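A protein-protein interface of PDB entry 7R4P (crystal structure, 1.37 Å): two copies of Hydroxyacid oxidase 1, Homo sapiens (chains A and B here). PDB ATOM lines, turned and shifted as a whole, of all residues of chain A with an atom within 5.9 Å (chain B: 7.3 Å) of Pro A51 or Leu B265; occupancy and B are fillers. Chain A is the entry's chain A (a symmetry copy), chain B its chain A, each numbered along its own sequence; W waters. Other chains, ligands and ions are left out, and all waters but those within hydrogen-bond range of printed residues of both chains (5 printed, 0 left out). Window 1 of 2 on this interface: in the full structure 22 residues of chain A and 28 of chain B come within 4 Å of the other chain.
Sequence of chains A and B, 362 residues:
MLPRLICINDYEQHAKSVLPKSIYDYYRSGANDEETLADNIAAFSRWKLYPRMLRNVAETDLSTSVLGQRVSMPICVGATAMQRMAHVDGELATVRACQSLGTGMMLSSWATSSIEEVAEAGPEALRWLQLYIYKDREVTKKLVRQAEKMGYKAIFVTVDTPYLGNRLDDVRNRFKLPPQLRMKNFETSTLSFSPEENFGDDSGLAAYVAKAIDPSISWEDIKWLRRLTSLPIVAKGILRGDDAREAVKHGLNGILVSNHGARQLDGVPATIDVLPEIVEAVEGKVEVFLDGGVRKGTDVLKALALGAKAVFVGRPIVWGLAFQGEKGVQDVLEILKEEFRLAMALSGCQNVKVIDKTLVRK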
ATOM      1  N   LEU A  49     -10.071   0.807  20.799  1.00  0.00           N
ATOM      2  CA  LEU A  49     -10.141  -0.669  20.689  1.00  0.00           C
ATOM      3  C   LEU A  49      -8.806  -1.269  20.231  1.00  0.00           C
ATOM      4  O   LEU A  49      -8.187  -0.714  19.337  1.00  0.00           O
ATOM      5  CB  LEU A  49     -11.254  -1.024  19.701  1.00  0.00           C
ATOM      6  CG  LEU A  49     -12.672  -0.820  20.237  1.00  0.00           C
ATOM      7  CD1 LEU A  49     -13.684  -0.785  19.104  1.00  0.00           C
ATOM      8  CD2 LEU A  49     -13.038  -1.895  21.247  1.00  0.00           C
ATOM      9  N   TYR A  50      -8.451  -2.395  20.831  1.00  0.00           N
ATOM     10  CA  TYR A  50      -7.190  -3.105  20.521  1.00  0.00           C
ATOM     11  C   TYR A  50      -7.593  -4.488  20.047  1.00  0.00           C
ATOM     12  O   TYR A  50      -7.597  -5.424  20.830  1.00  0.00           O
ATOM     13  CB  TYR A  50      -6.317  -3.139  21.769  1.00  0.00           C
ATOM     14  CG  TYR A  50      -5.747  -1.778  22.064  1.00  0.00           C
ATOM     15  CD1 TYR A  50      -6.526  -0.789  22.634  1.00  0.00           C
ATOM     16  CD2 TYR A  50      -4.456  -1.453  21.693  1.00  0.00           C
ATOM     17  CE1 TYR A  50      -6.030   0.481  22.859  1.00  0.00           C
ATOM     18  CE2 TYR A  50      -3.940  -0.190  21.917  1.00  0.00           C
ATOM     19  CZ  TYR A  50      -4.728   0.778  22.507  1.00  0.00           C
ATOM     20  OH  TYR A  50      -4.225   2.023  22.740  1.00  0.00           O
ATOM     21  N   PRO A  51      -7.972  -4.614  18.767  1.00  0.00           N
ATOM     22  CA  PRO A  51      -8.506  -5.869  18.269  1.00  0.00           C
ATOM     23  C   PRO A  51      -7.494  -7.002  18.082  1.00  0.00           C
ATOM     24  O   PRO A  51      -6.377  -6.747  17.760  1.00  0.00           O
ATOM     25  CB  PRO A  51      -9.081  -5.477  16.895  1.00  0.00           C
ATOM     26  CG  PRO A  51      -8.209  -4.327  16.457  1.00  0.00           C
ATOM     27  CD  PRO A  51      -7.916  -3.575  17.738  1.00  0.00           C
ATOM     28  N   ARG A  52      -7.933  -8.203  18.411  1.00  0.00           N
ATOM     29  CA  ARG A  52      -7.144  -9.387  18.114  1.00  0.00           C
ATOM     30  C   ARG A  52      -7.430  -9.950  16.719  1.00  0.00           C
ATOM     31  O   ARG A  52      -8.646  -9.888  16.294  1.00  0.00           O
ATOM     32  CB  ARG A  52      -7.507 -10.488  19.107  1.00  0.00           C
ATOM     33  CG  ARG A  52      -6.972 -10.227  20.519  1.00  0.00           C
ATOM     34  CD  ARG A  52      -7.132 -11.529  21.303  1.00  0.00           C
ATOM     35  NE  ARG A  52      -6.796 -11.394  22.700  1.00  0.00           N
ATOM     36  CZ  ARG A  52      -7.576 -10.906  23.652  1.00  0.00           C
ATOM     37  NH1 ARG A  52      -7.121 -10.890  24.902  1.00  0.00           N
ATOM     38  NH2 ARG A  52      -8.769 -10.419  23.379  1.00  0.00           N
ATOM     39  N   MET A  53      -6.407 -10.389  16.038  1.00  0.00           N
ATOM     40  CA  MET A  53      -6.546 -10.910  14.671  1.00  0.00           C
ATOM     41  C   MET A  53      -6.563 -12.437  14.720  1.00  0.00           C
ATOM     42  O   MET A  53      -5.985 -13.070  15.649  1.00  0.00           O
ATOM     43  CB  MET A  53      -5.409 -10.379  13.785  1.00  0.00           C
ATOM     44  CG  MET A  53      -5.330  -8.806  13.815  1.00  0.00           C
ATOM     45  SD  MET A  53      -6.848  -8.092  13.325  1.00  0.00           S
ATOM     46  CE  MET A  53      -6.623  -6.420  13.952  1.00  0.00           C
ATOM     47  N   THR A 298     -19.730  -0.426  18.174  1.00  0.00           N
ATOM     48  CA  THR A 298     -18.469  -0.336  18.935  1.00  0.00           C
ATOM     49  C   THR A 298     -18.752   0.215  20.338  1.00  0.00           C
ATOM     50  O   THR A 298     -17.990  -0.079  21.240  1.00  0.00           O
ATOM     51  CB  THR A 298     -17.386   0.486  18.184  1.00  0.00           C
ATOM     52  OG1 THR A 298     -17.991   1.722  17.760  1.00  0.00           O
ATOM     53  CG2 THR A 298     -16.816  -0.250  16.983  1.00  0.00           C
ATOM     54  N   LEU A 301     -19.588  -2.841  22.313  1.00  0.00           N
ATOM     55  CA  LEU A 301     -18.383  -3.635  22.534  1.00  0.00           C
ATOM     56  C   LEU A 301     -17.536  -3.043  23.661  1.00  0.00           C
ATOM     57  O   LEU A 301     -17.051  -3.757  24.523  1.00  0.00           O
ATOM     58  CB  LEU A 301     -17.590  -3.762  21.225  1.00  0.00           C
ATOM     59  CG  LEU A 301     -16.322  -4.554  21.298  1.00  0.00           C
ATOM     60  CD1 LEU A 301     -16.641  -6.008  21.638  1.00  0.00           C
ATOM     61  CD2 LEU A 301     -15.574  -4.490  19.974  1.00  0.00           C
ATOM     62  N   LEU A 342     -20.370  -7.045  13.695  1.00  0.00           N
ATOM     63  CA  LEU A 342     -19.149  -6.688  12.924  1.00  0.00           C
ATOM     64  C   LEU A 342     -18.020  -6.274  13.876  1.00  0.00           C
ATOM     65  O   LEU A 342     -16.917  -6.724  13.691  1.00  0.00           O
ATOM     66  CB  LEU A 342     -19.503  -5.597  11.920  1.00  0.00           C
ATOM     67  CG  LEU A 342     -18.368  -5.229  10.969  1.00  0.00           C
ATOM     68  CD1 LEU A 342     -17.908  -6.452  10.188  1.00  0.00           C
ATOM     69  CD2 LEU A 342     -18.798  -4.118  10.027  1.00  0.00           C
ATOM     70  N   ALA A 343     -18.338  -5.461  14.873  1.00  0.00           N
ATOM     71  CA  ALA A 343     -17.289  -4.986  15.795  1.00  0.00           C
ATOM     72  C   ALA A 343     -16.711  -6.176  16.562  1.00  0.00           C
ATOM     73  O   ALA A 343     -15.509  -6.250  16.714  1.00  0.00           O
ATOM     74  CB  ALA A 343     -17.884  -3.954  16.719  1.00  0.00           C
ATOM     75  N   LEU A 346     -14.518  -8.113  14.008  1.00  0.00           N
ATOM     76  CA  LEU A 346     -13.254  -7.433  13.640  1.00  0.00           C
ATOM     77  C   LEU A 346     -12.320  -7.345  14.842  1.00  0.00           C
ATOM     78  O   LEU A 346     -11.119  -7.316  14.637  1.00  0.00           O
ATOM     79  CB  LEU A 346     -13.585  -6.050  13.081  1.00  0.00           C
ATOM     80  CG  LEU A 346     -14.386  -6.021  11.783  1.00  0.00           C
ATOM     81  CD1 LEU A 346     -14.578  -4.588  11.311  1.00  0.00           C
ATOM     82  CD2 LEU A 346     -13.704  -6.847  10.705  1.00  0.00           C
ATOM     83  N   SER A 347     -12.861  -7.556  16.045  1.00  0.00           N
ATOM     84  CA  SER A 347     -12.033  -7.491  17.281  1.00  0.00           C
ATOM     85  C   SER A 347     -11.528  -8.886  17.665  1.00  0.00           C
ATOM     86  O   SER A 347     -10.841  -9.002  18.691  1.00  0.00           O
ATOM     87  CB  SER A 347     -12.793  -6.836  18.411  1.00  0.00           C
ATOM     88  OG  SER A 347     -13.918  -7.611  18.789  1.00  0.00           O
ATOM     89  N   GLY A 348     -12.026  -9.923  16.984  1.00  0.00           N
ATOM     90  CA  GLY A 348     -11.578 -11.310  17.268  1.00  0.00           C
ATOM     91  C   GLY A 348     -12.443 -12.038  18.274  1.00  0.00           C
ATOM     92  O   GLY A 348     -11.988 -13.013  18.827  1.00  0.00           O
ATOM     93  N   LEU A 359      -9.262  -5.506  25.322  1.00  0.00           N
ATOM     94  CA  LEU A 359      -9.771  -4.920  24.090  1.00  0.00           C
ATOM     95  C   LEU A 359      -9.797  -3.397  24.164  1.00  0.00           C
ATOM     96  O   LEU A 359      -9.985  -2.781  23.095  1.00  0.00           O
ATOM     97  CB  LEU A 359     -11.155  -5.452  23.781  1.00  0.00           C
ATOM     98  CG  LEU A 359     -11.184  -6.876  23.317  1.00  0.00           C
ATOM     99  CD1 LEU A 359     -12.632  -7.286  23.190  1.00  0.00           C
ATOM    100  CD2 LEU A 359     -10.504  -7.081  21.969  1.00  0.00           C
ATOM    101  N   ALA B  31     -14.103   3.715   8.100  1.00  0.00           N
ATOM    102  CA  ALA B  31     -15.254   2.969   8.636  1.00  0.00           C
ATOM    103  C   ALA B  31     -16.119   3.811   9.580  1.00  0.00           C
ATOM    104  O   ALA B  31     -15.581   4.598  10.331  1.00  0.00           O
ATOM    105  CB  ALA B  31     -14.766   1.732   9.352  1.00  0.00           C
ATOM    106  N   ASN B  32     -17.431   3.643   9.481  1.00  0.00           N
ATOM    107  CA  ASN B  32     -18.389   4.203  10.449  1.00  0.00           C
ATOM    108  C   ASN B  32     -18.155   5.685  10.571  1.00  0.00           C
ATOM    109  O   ASN B  32     -18.207   6.401   9.545  1.00  0.00           O
ATOM    110  CB  ASN B  32     -18.372   3.388  11.754  1.00  0.00           C
ATOM    111  CG  ASN B  32     -18.725   1.942  11.551  1.00  0.00           C
ATOM    112  OD1 ASN B  32     -19.913   1.577  11.542  1.00  0.00           O
ATOM    113  ND2 ASN B  32     -17.714   1.183  11.373  1.00  0.00           N
ATOM    114  N   THR B  36     -10.956   6.895  13.525  1.00  0.00           N
ATOM    115  CA  THR B  36      -9.574   6.469  13.298  1.00  0.00           C
ATOM    116  C   THR B  36      -9.026   7.162  12.051  1.00  0.00           C
ATOM    117  O   THR B  36      -7.823   7.453  12.014  1.00  0.00           O
ATOM    118  CB  THR B  36      -9.495   4.952  13.215  1.00  0.00           C
ATOM    119  OG1 THR B  36      -9.971   4.360  14.441  1.00  0.00           O
ATOM    120  CG2 THR B  36      -8.128   4.423  12.949  1.00  0.00           C
ATOM    121  N   ASP B 160      -6.598  -8.447   9.108  1.00  0.00           N
ATOM    122  CA  ASP B 160      -7.589  -7.627   9.848  1.00  0.00           C
ATOM    123  C   ASP B 160      -8.949  -7.598   9.179  1.00  0.00           C
ATOM    124  O   ASP B 160      -9.799  -6.737   9.539  1.00  0.00           O
ATOM    125  CB  ASP B 160      -7.061  -6.213  10.038  1.00  0.00           C
ATOM    126  CG  ASP B 160      -6.716  -5.429   8.782  1.00  0.00           C
ATOM    127  OD1 ASP B 160      -7.081  -5.895   7.678  1.00  0.00           O
ATOM    128  OD2 ASP B 160      -6.100  -4.324   8.885  1.00  0.00           O
ATOM    129  N   TYR B 163     -14.202  -9.919   7.794  1.00  0.00           N
ATOM    130  CA  TYR B 163     -15.332  -9.265   7.097  1.00  0.00           C
ATOM    131  C   TYR B 163     -14.845  -7.886   6.695  1.00  0.00           C
ATOM    132  O   TYR B 163     -13.907  -7.358   7.337  1.00  0.00           O
ATOM    133  CB  TYR B 163     -16.553  -9.126   8.016  1.00  0.00           C
ATOM    134  CG  TYR B 163     -17.099 -10.444   8.501  1.00  0.00           C
ATOM    135  CD1 TYR B 163     -18.009 -11.206   7.758  1.00  0.00           C
ATOM    136  CD2 TYR B 163     -16.710 -10.998   9.728  1.00  0.00           C
ATOM    137  CE1 TYR B 163     -18.475 -12.409   8.213  1.00  0.00           C
ATOM    138  CE2 TYR B 163     -17.167 -12.221  10.180  1.00  0.00           C
ATOM    139  CZ  TYR B 163     -18.047 -12.962   9.416  1.00  0.00           C
ATOM    140  OH  TYR B 163     -18.549 -14.147   9.864  1.00  0.00           O
ATOM    141  N   LEU B 164     -15.484  -7.263   5.733  1.00  0.00           N
ATOM    142  CA  LEU B 164     -15.169  -5.876   5.382  1.00  0.00           C
ATOM    143  C   LEU B 164     -15.770  -4.901   6.423  1.00  0.00           C
ATOM    144  O   LEU B 164     -16.890  -5.059   6.887  1.00  0.00           O
ATOM    145  CB  LEU B 164     -15.844  -5.572   4.031  1.00  0.00           C
ATOM    146  N   GLY B 165     -14.993  -3.863   6.673  1.00  0.00           N
ATOM    147  CA  GLY B 165     -15.526  -2.730   7.433  1.00  0.00           C
ATOM    148  C   GLY B 165     -16.719  -2.091   6.794  1.00  0.00           C
ATOM    149  O   GLY B 165     -16.934  -2.163   5.544  1.00  0.00           O
ATOM    150  N   ASN B 166     -17.497  -1.394   7.608  1.00  0.00           N
ATOM    151  CA  ASN B 166     -18.717  -0.683   7.149  1.00  0.00           C
ATOM    152  C   ASN B 166     -18.377   0.767   6.777  1.00  0.00           C
ATOM    153  O   ASN B 166     -18.329   1.608   7.676  1.00  0.00           O
ATOM    154  CB  ASN B 166     -19.803  -0.771   8.219  1.00  0.00           C
ATOM    155  CG  ASN B 166     -21.104  -0.107   7.831  1.00  0.00           C
ATOM    156  OD1 ASN B 166     -21.409   0.035   6.654  1.00  0.00           O
ATOM    157  ND2 ASN B 166     -21.875   0.299   8.823  1.00  0.00           N
ATOM    158  N   ARG B 167     -18.105   1.004   5.497  1.00  0.00           N
ATOM    159  CA  ARG B 167     -17.836   2.387   5.003  1.00  0.00           C
ATOM    160  C   ARG B 167     -19.184   2.980   4.522  1.00  0.00           C
ATOM    161  O   ARG B 167     -19.879   2.602   3.474  1.00  0.00           O
ATOM    162  CB  ARG B 167     -16.757   2.367   3.918  1.00  0.00           C
ATOM    163  CG  ARG B 167     -15.385   1.958   4.430  1.00  0.00           C
ATOM    164  CD  ARG B 167     -14.322   1.852   3.350  1.00  0.00           C
ATOM    165  NE  ARG B 167     -14.330   0.555   2.689  1.00  0.00           N
ATOM    166  CZ  ARG B 167     -14.150  -0.604   3.315  1.00  0.00           C
ATOM    167  NH1 ARG B 167     -13.951  -0.632   4.619  1.00  0.00           N
ATOM    168  NH2 ARG B 167     -14.187  -1.738   2.642  1.00  0.00           N
ATOM    169  N   GLY B 237      -1.781  -5.577   9.272  1.00  0.00           N
ATOM    170  CA  GLY B 237      -2.985  -5.237  10.070  1.00  0.00           C
ATOM    171  C   GLY B 237      -2.924  -5.606  11.527  1.00  0.00           C
ATOM    172  O   GLY B 237      -3.976  -5.465  12.244  1.00  0.00           O
ATOM    173  N   ILE B 238      -1.763  -5.891  12.014  1.00  0.00           N
ATOM    174  CA  ILE B 238      -1.496  -6.103  13.456  1.00  0.00           C
ATOM    175  C   ILE B 238      -1.530  -4.797  14.220  1.00  0.00           C
ATOM    176  O   ILE B 238      -0.830  -3.880  13.846  1.00  0.00           O
ATOM    177  CB  ILE B 238      -0.123  -6.757  13.611  1.00  0.00           C
ATOM    178  CG1 ILE B 238      -0.048  -8.100  12.869  1.00  0.00           C
ATOM    179  CG2 ILE B 238       0.263  -6.861  15.077  1.00  0.00           C
ATOM    180  CD1 ILE B 238      -0.927  -9.201  13.429  1.00  0.00           C
ATOM    181  N   LEU B 239      -2.223  -4.771  15.353  1.00  0.00           N
ATOM    182  CA  LEU B 239      -2.358  -3.606  16.228  1.00  0.00           C
ATOM    183  C   LEU B 239      -1.972  -3.928  17.646  1.00  0.00           C
ATOM    184  O   LEU B 239      -1.930  -2.942  18.405  1.00  0.00           O
ATOM    185  CB  LEU B 239      -3.777  -3.033  16.105  1.00  0.00           C
ATOM    186  CG  LEU B 239      -4.115  -2.410  14.758  1.00  0.00           C
ATOM    187  CD1 LEU B 239      -5.613  -2.103  14.689  1.00  0.00           C
ATOM    188  CD2 LEU B 239      -3.250  -1.188  14.484  1.00  0.00           C
ATOM    189  N   ARG B 240      -1.704  -5.133  18.062  1.00  0.00           N
ATOM    190  CA  ARG B 240      -1.416  -5.566  19.433  1.00  0.00           C
ATOM    191  C   ARG B 240      -0.038  -6.201  19.499  1.00  0.00           C
ATOM    192  O   ARG B 240       0.308  -7.016  18.635  1.00  0.00           O
ATOM    193  CB  ARG B 240      -2.441  -6.571  19.908  1.00  0.00           C
ATOM    194  CG  ARG B 240      -3.859  -6.033  20.106  1.00  0.00           C
ATOM    195  CD  ARG B 240      -4.750  -7.179  20.421  1.00  0.00           C
ATOM    196  NE  ARG B 240      -4.464  -7.822  21.678  1.00  0.00           N
ATOM    197  CZ  ARG B 240      -5.166  -7.727  22.804  1.00  0.00           C
ATOM    198  NH1 ARG B 240      -4.796  -8.415  23.845  1.00  0.00           N
ATOM    199  NH2 ARG B 240      -6.263  -6.974  22.885  1.00  0.00           N
ATOM    200  N   ASP B 242       0.856  -8.609  21.520  1.00  0.00           N
ATOM    201  CA  ASP B 242       0.742 -10.071  21.680  1.00  0.00           C
ATOM    202  C   ASP B 242       0.561 -10.736  20.319  1.00  0.00           C
ATOM    203  O   ASP B 242       1.184 -11.752  20.055  1.00  0.00           O
ATOM    204  CB  ASP B 242      -0.317 -10.466  22.687  1.00  0.00           C
ATOM    205  CG  ASP B 242      -1.739  -9.930  22.533  1.00  0.00           C
ATOM    206  OD1 ASP B 242      -2.067  -9.315  21.521  1.00  0.00           O
ATOM    207  OD2 ASP B 242      -2.486 -10.187  23.507  1.00  0.00           O
ATOM    208  N   ASP B 243      -0.254 -10.171  19.450  1.00  0.00           N
ATOM    209  CA  ASP B 243      -0.421 -10.675  18.063  1.00  0.00           C
ATOM    210  C   ASP B 243       0.893 -10.540  17.282  1.00  0.00           C
ATOM    211  O   ASP B 243       1.227 -11.485  16.533  1.00  0.00           O
ATOM    212  CB  ASP B 243      -1.555  -9.967  17.348  1.00  0.00           C
ATOM    213  CG  ASP B 243      -2.948 -10.415  17.717  1.00  0.00           C
ATOM    214  OD1 ASP B 243      -3.095 -11.370  18.464  1.00  0.00           O
ATOM    215  OD2 ASP B 243      -3.861  -9.779  17.127  1.00  0.00           O
ATOM    216  N   ASN B 259      -4.053  -0.197  10.391  1.00  0.00           N
ATOM    217  CA  ASN B 259      -5.506  -0.277  10.669  1.00  0.00           C
ATOM    218  C   ASN B 259      -6.273  -0.260   9.363  1.00  0.00           C
ATOM    219  O   ASN B 259      -7.459   0.090   9.340  1.00  0.00           O
ATOM    220  CB  ASN B 259      -5.981   0.747  11.688  1.00  0.00           C
ATOM    221  CG  ASN B 259      -5.556   2.153  11.352  1.00  0.00           C
ATOM    222  OD1 ASN B 259      -5.492   2.503  10.178  1.00  0.00           O
ATOM    223  ND2 ASN B 259      -5.241   2.958  12.385  1.00  0.00           N
ATOM    224  N   HIS B 260      -5.609  -0.678   8.299  1.00  0.00           N
ATOM    225  CA  HIS B 260      -6.262  -0.852   6.967  1.00  0.00           C
ATOM    226  C   HIS B 260      -6.761   0.514   6.458  1.00  0.00           C
ATOM    227  O   HIS B 260      -7.849   0.663   5.922  1.00  0.00           O
ATOM    228  CB  HIS B 260      -7.354  -1.896   7.063  1.00  0.00           C
ATOM    229  CG  HIS B 260      -7.693  -2.603   5.794  1.00  0.00           C
ATOM    230  ND1 HIS B 260      -7.639  -3.976   5.740  1.00  0.00           N
ATOM    231  CD2 HIS B 260      -8.274  -2.157   4.651  1.00  0.00           C
ATOM    232  CE1 HIS B 260      -8.090  -4.311   4.499  1.00  0.00           C
ATOM    233  NE2 HIS B 260      -8.466  -3.259   3.840  1.00  0.00           N
ATOM    234  N   ALA B 262      -7.850   2.853   8.212  1.00  0.00           N
ATOM    235  CA  ALA B 262      -8.984   3.213   9.073  1.00  0.00           C
ATOM    236  C   ALA B 262     -10.303   2.745   8.470  1.00  0.00           C
ATOM    237  O   ALA B 262     -11.360   3.346   8.711  1.00  0.00           O
ATOM    238  CB  ALA B 262      -8.986   4.690   9.365  1.00  0.00           C
ATOM    239  N   ARG B 263     -10.251   1.680   7.666  1.00  0.00           N
ATOM    240  CA  ARG B 263     -11.449   1.233   6.902  1.00  0.00           C
ATOM    241  C   ARG B 263     -12.057  -0.048   7.478  1.00  0.00           C
ATOM    242  O   ARG B 263     -13.034  -0.525   6.913  1.00  0.00           O
ATOM    243  CB  ARG B 263     -11.049   0.969   5.446  1.00  0.00           C
ATOM    244  CG  ARG B 263     -10.717   2.230   4.666  1.00  0.00           C
ATOM    245  CD  ARG B 263      -9.854   1.953   3.453  1.00  0.00           C
ATOM    246  NE  ARG B 263     -10.535   1.396   2.294  1.00  0.00           N
ATOM    247  CZ  ARG B 263     -11.234   2.098   1.412  1.00  0.00           C
ATOM    248  NH1 ARG B 263     -11.401   3.399   1.573  1.00  0.00           N
ATOM    249  NH2 ARG B 263     -11.774   1.496   0.370  1.00  0.00           N
ATOM    250  N   GLN B 264     -11.486  -0.565   8.551  1.00  0.00           N
ATOM    251  CA  GLN B 264     -11.997  -1.834   9.120  1.00  0.00           C
ATOM    252  C   GLN B 264     -12.740  -1.536  10.434  1.00  0.00           C
ATOM    253  O   GLN B 264     -13.885  -1.153  10.367  1.00  0.00           O
ATOM    254  CB  GLN B 264     -10.838  -2.816   9.256  1.00  0.00           C
ATOM    255  CG  GLN B 264     -10.457  -3.470   7.932  1.00  0.00           C
ATOM    256  CD  GLN B 264     -11.602  -4.247   7.325  1.00  0.00           C
ATOM    257  OE1 GLN B 264     -12.187  -3.849   6.324  1.00  0.00           O
ATOM    258  NE2 GLN B 264     -11.938  -5.361   7.947  1.00  0.00           N
ATOM    259  N   LEU B 265     -12.064  -1.730  11.563  1.00  0.00           N
ATOM    260  CA  LEU B 265     -12.674  -1.405  12.880  1.00  0.00           C
ATOM    261  C   LEU B 265     -12.409   0.068  13.227  1.00  0.00           C
ATOM    262  O   LEU B 265     -11.268   0.455  13.345  1.00  0.00           O
ATOM    263  CB  LEU B 265     -12.111  -2.364  13.934  1.00  0.00           C
ATOM    264  CG  LEU B 265     -12.695  -2.210  15.336  1.00  0.00           C
ATOM    265  CD1 LEU B 265     -14.201  -2.418  15.317  1.00  0.00           C
ATOM    266  CD2 LEU B 265     -12.034  -3.184  16.296  1.00  0.00           C
ATOM    267  N   ASP B 266     -13.481   0.842  13.337  1.00  0.00           N
ATOM    268  CA  ASP B 266     -13.320   2.257  13.747  1.00  0.00           C
ATOM    269  C   ASP B 266     -13.130   2.336  15.254  1.00  0.00           C
ATOM    270  O   ASP B 266     -13.749   1.568  15.976  1.00  0.00           O
ATOM    271  CB  ASP B 266     -14.467   3.160  13.290  1.00  0.00           C
ATOM    272  CG  ASP B 266     -14.096   4.634  13.328  1.00  0.00           C
ATOM    273  OD1 ASP B 266     -12.954   4.951  12.981  1.00  0.00           O
ATOM    274  OD2 ASP B 266     -14.953   5.443  13.709  1.00  0.00           O
ATOM    275  N   GLY B 267     -12.283   3.259  15.654  1.00  0.00           N
ATOM    276  CA  GLY B 267     -12.001   3.471  17.070  1.00  0.00           C
ATOM    277  C   GLY B 267     -10.762   2.738  17.501  1.00  0.00           C
ATOM    278  O   GLY B 267     -10.516   2.757  18.721  1.00  0.00           O
ATOM    279  N   VAL B 268     -10.049   2.064  16.651  1.00  0.00           N
ATOM    280  CA  VAL B 268      -8.681   1.633  16.983  1.00  0.00           C
ATOM    281  C   VAL B 268      -7.770   2.835  16.983  1.00  0.00           C
ATOM    282  O   VAL B 268      -8.076   3.885  16.419  1.00  0.00           O
ATOM    283  CB  VAL B 268      -8.240   0.531  16.023  1.00  0.00           C
ATOM    284  CG1 VAL B 268      -9.214  -0.599  16.013  1.00  0.00           C
ATOM    285  CG2 VAL B 268      -8.062   1.075  14.595  1.00  0.00           C
ATOM    286  N   PRO B 269      -6.621   2.713  17.653  1.00  0.00           N
ATOM    287  CA  PRO B 269      -5.685   3.822  17.668  1.00  0.00           C
ATOM    288  C   PRO B 269      -5.069   4.059  16.297  1.00  0.00           C
ATOM    289  O   PRO B 269      -5.102   3.234  15.369  1.00  0.00           O
ATOM    290  CB  PRO B 269      -4.583   3.364  18.605  1.00  0.00           C
ATOM    291  CG  PRO B 269      -5.121   2.241  19.311  1.00  0.00           C
ATOM    292  CD  PRO B 269      -6.099   1.550  18.378  1.00  0.00           C
HETATM  293  O   HOH W   1      -3.714  -7.077  16.593  1.00  0.00           O
HETATM  294  O   HOH W   2      -4.657 -13.424  17.880  1.00  0.00           O
HETATM  295  O   HOH W   3      -9.991  -5.808  12.292  1.00  0.00           O
HETATM  296  O   HOH W   4     -15.072   2.985  18.037  1.00  0.00           O
HETATM  297  O   HOH W   5      -4.202 -12.414  22.813  1.00  0.00           O
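The backbone NH of Met A53 lies within hydrogen-bond range of the side-chain carboxylate of Asp B243, at 2.8 Å.
O of Tyr A50 is in hydrogen-bond range of NH2 of Arg B240.
O of Gly B267 lies within hydrogen-bond range of N of Leu A49, 2.9 Å away.
The side-chain hydroxyl (OG1) of Thr B36 sits at hydrogen-bond distance from the backbone NH (N) of Gly B267 (2.8 Å).
The side-chain amide oxygen (OE1) of Gln B264 lies within hydrogen-bond range of the backbone NH (N) of Gly B165 (2.8 Å).
O of Tyr B163 sits at hydrogen-bond distance from NE2 of Gln B264.
The backbone NH of Asn B32 lies within hydrogen-bond range of the backbone carbonyl oxygen of Asn B166.
The side-chain carboxylate of Asp B242 lies within salt-bridge range of the guanidinium group of Arg B240 (2.8 Å).
O of Ser A347 lies within hydrogen-bond range of N of Arg A52 (3.0 Å).
Asp B266 touches Leu A49 (O to CD1, 3.9 Å).
Leu A49 touches Val B268.
Tyr A50 touches Pro B269 (CZ to CG, 3.5 Å).
CD1 of Leu B239 touches CG of Pro A51, at 3.8 Å.
CD of Pro A51 touches CG1 of Val B268, at 3.7 Å.
Asp B243 touches Arg A52.
Asp B160 touches Met A53.
CG2 of Thr A298 touches CD1 of Leu B265 (3.8 Å).
Thr A298 touches Asp B266.
Leu A346 touches Gln B264.
Of the printed residues of chain B, Pro A51 touches Leu B239 (3.8 Å), Arg B240 (3.1 Å), Asp B243 (3.99 Å), Leu B265 (3.8 Å) and Val B268 (3.7 Å).
Printed residues of chain A within 4 Å of Leu B265: Pro A51 (3.8 Å), Thr A298 (3.8 Å) and Leu A346 (3.8 Å).
Of the printed residues of chain A, Gly B267 touches Leu A49 (2.9 Å).
Printed residues of chain B within 4 Å of Met A53: Asp B160 (3.6 Å), Gly B237 (3.3 Å) and Asp B243 (2.8 Å).
Ala B31 touches none of the printed residues of chain A.
The nearest printed residue of chain B that does not touch Pro A51 is Pro B269 (5.5 Å).
The nearest printed residue of chain A that does not touch Leu B265 is Ala A343 (4.04 Å).
The nearest printed residue of chain A that does not touch Asp B160 is Leu A346 (4.1 Å).
Among the printed residues, no Asp or Glu carboxylate lies within 4 Å of a Lys or Arg side-chain nitrogen of the other chain.
No position is printed for both chains.
Of the 24 pairs that touch across the chains among the printed residues, none has its exchanged pair printed and touching as well.
Water W2 lies within hydrogen-bond range of O of Met A53 (2.6 Å) and OD1 of Asp B243 (2.6 Å).
Water W1 lies within hydrogen-bond range of OD2 of Asp B243 (2.8 Å), O of Pro A51 (2.9 Å), N of Leu B239 (3.0 Å) and N of Arg B240 (3.2 Å).
Water W5 lies within hydrogen-bond range of NE of Arg A52 (2.8 Å) and OD2 of Asp B242 (2.9 Å).
Water W4 lies within hydrogen-bond range of O of Asp B266 (2.8 Å) and OG1 of Thr A298 (3.2 Å).
Water W3 bridges the backbone carbonyl oxygen of Asp B160 and the backbone carbonyl oxygen of Leu A346.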
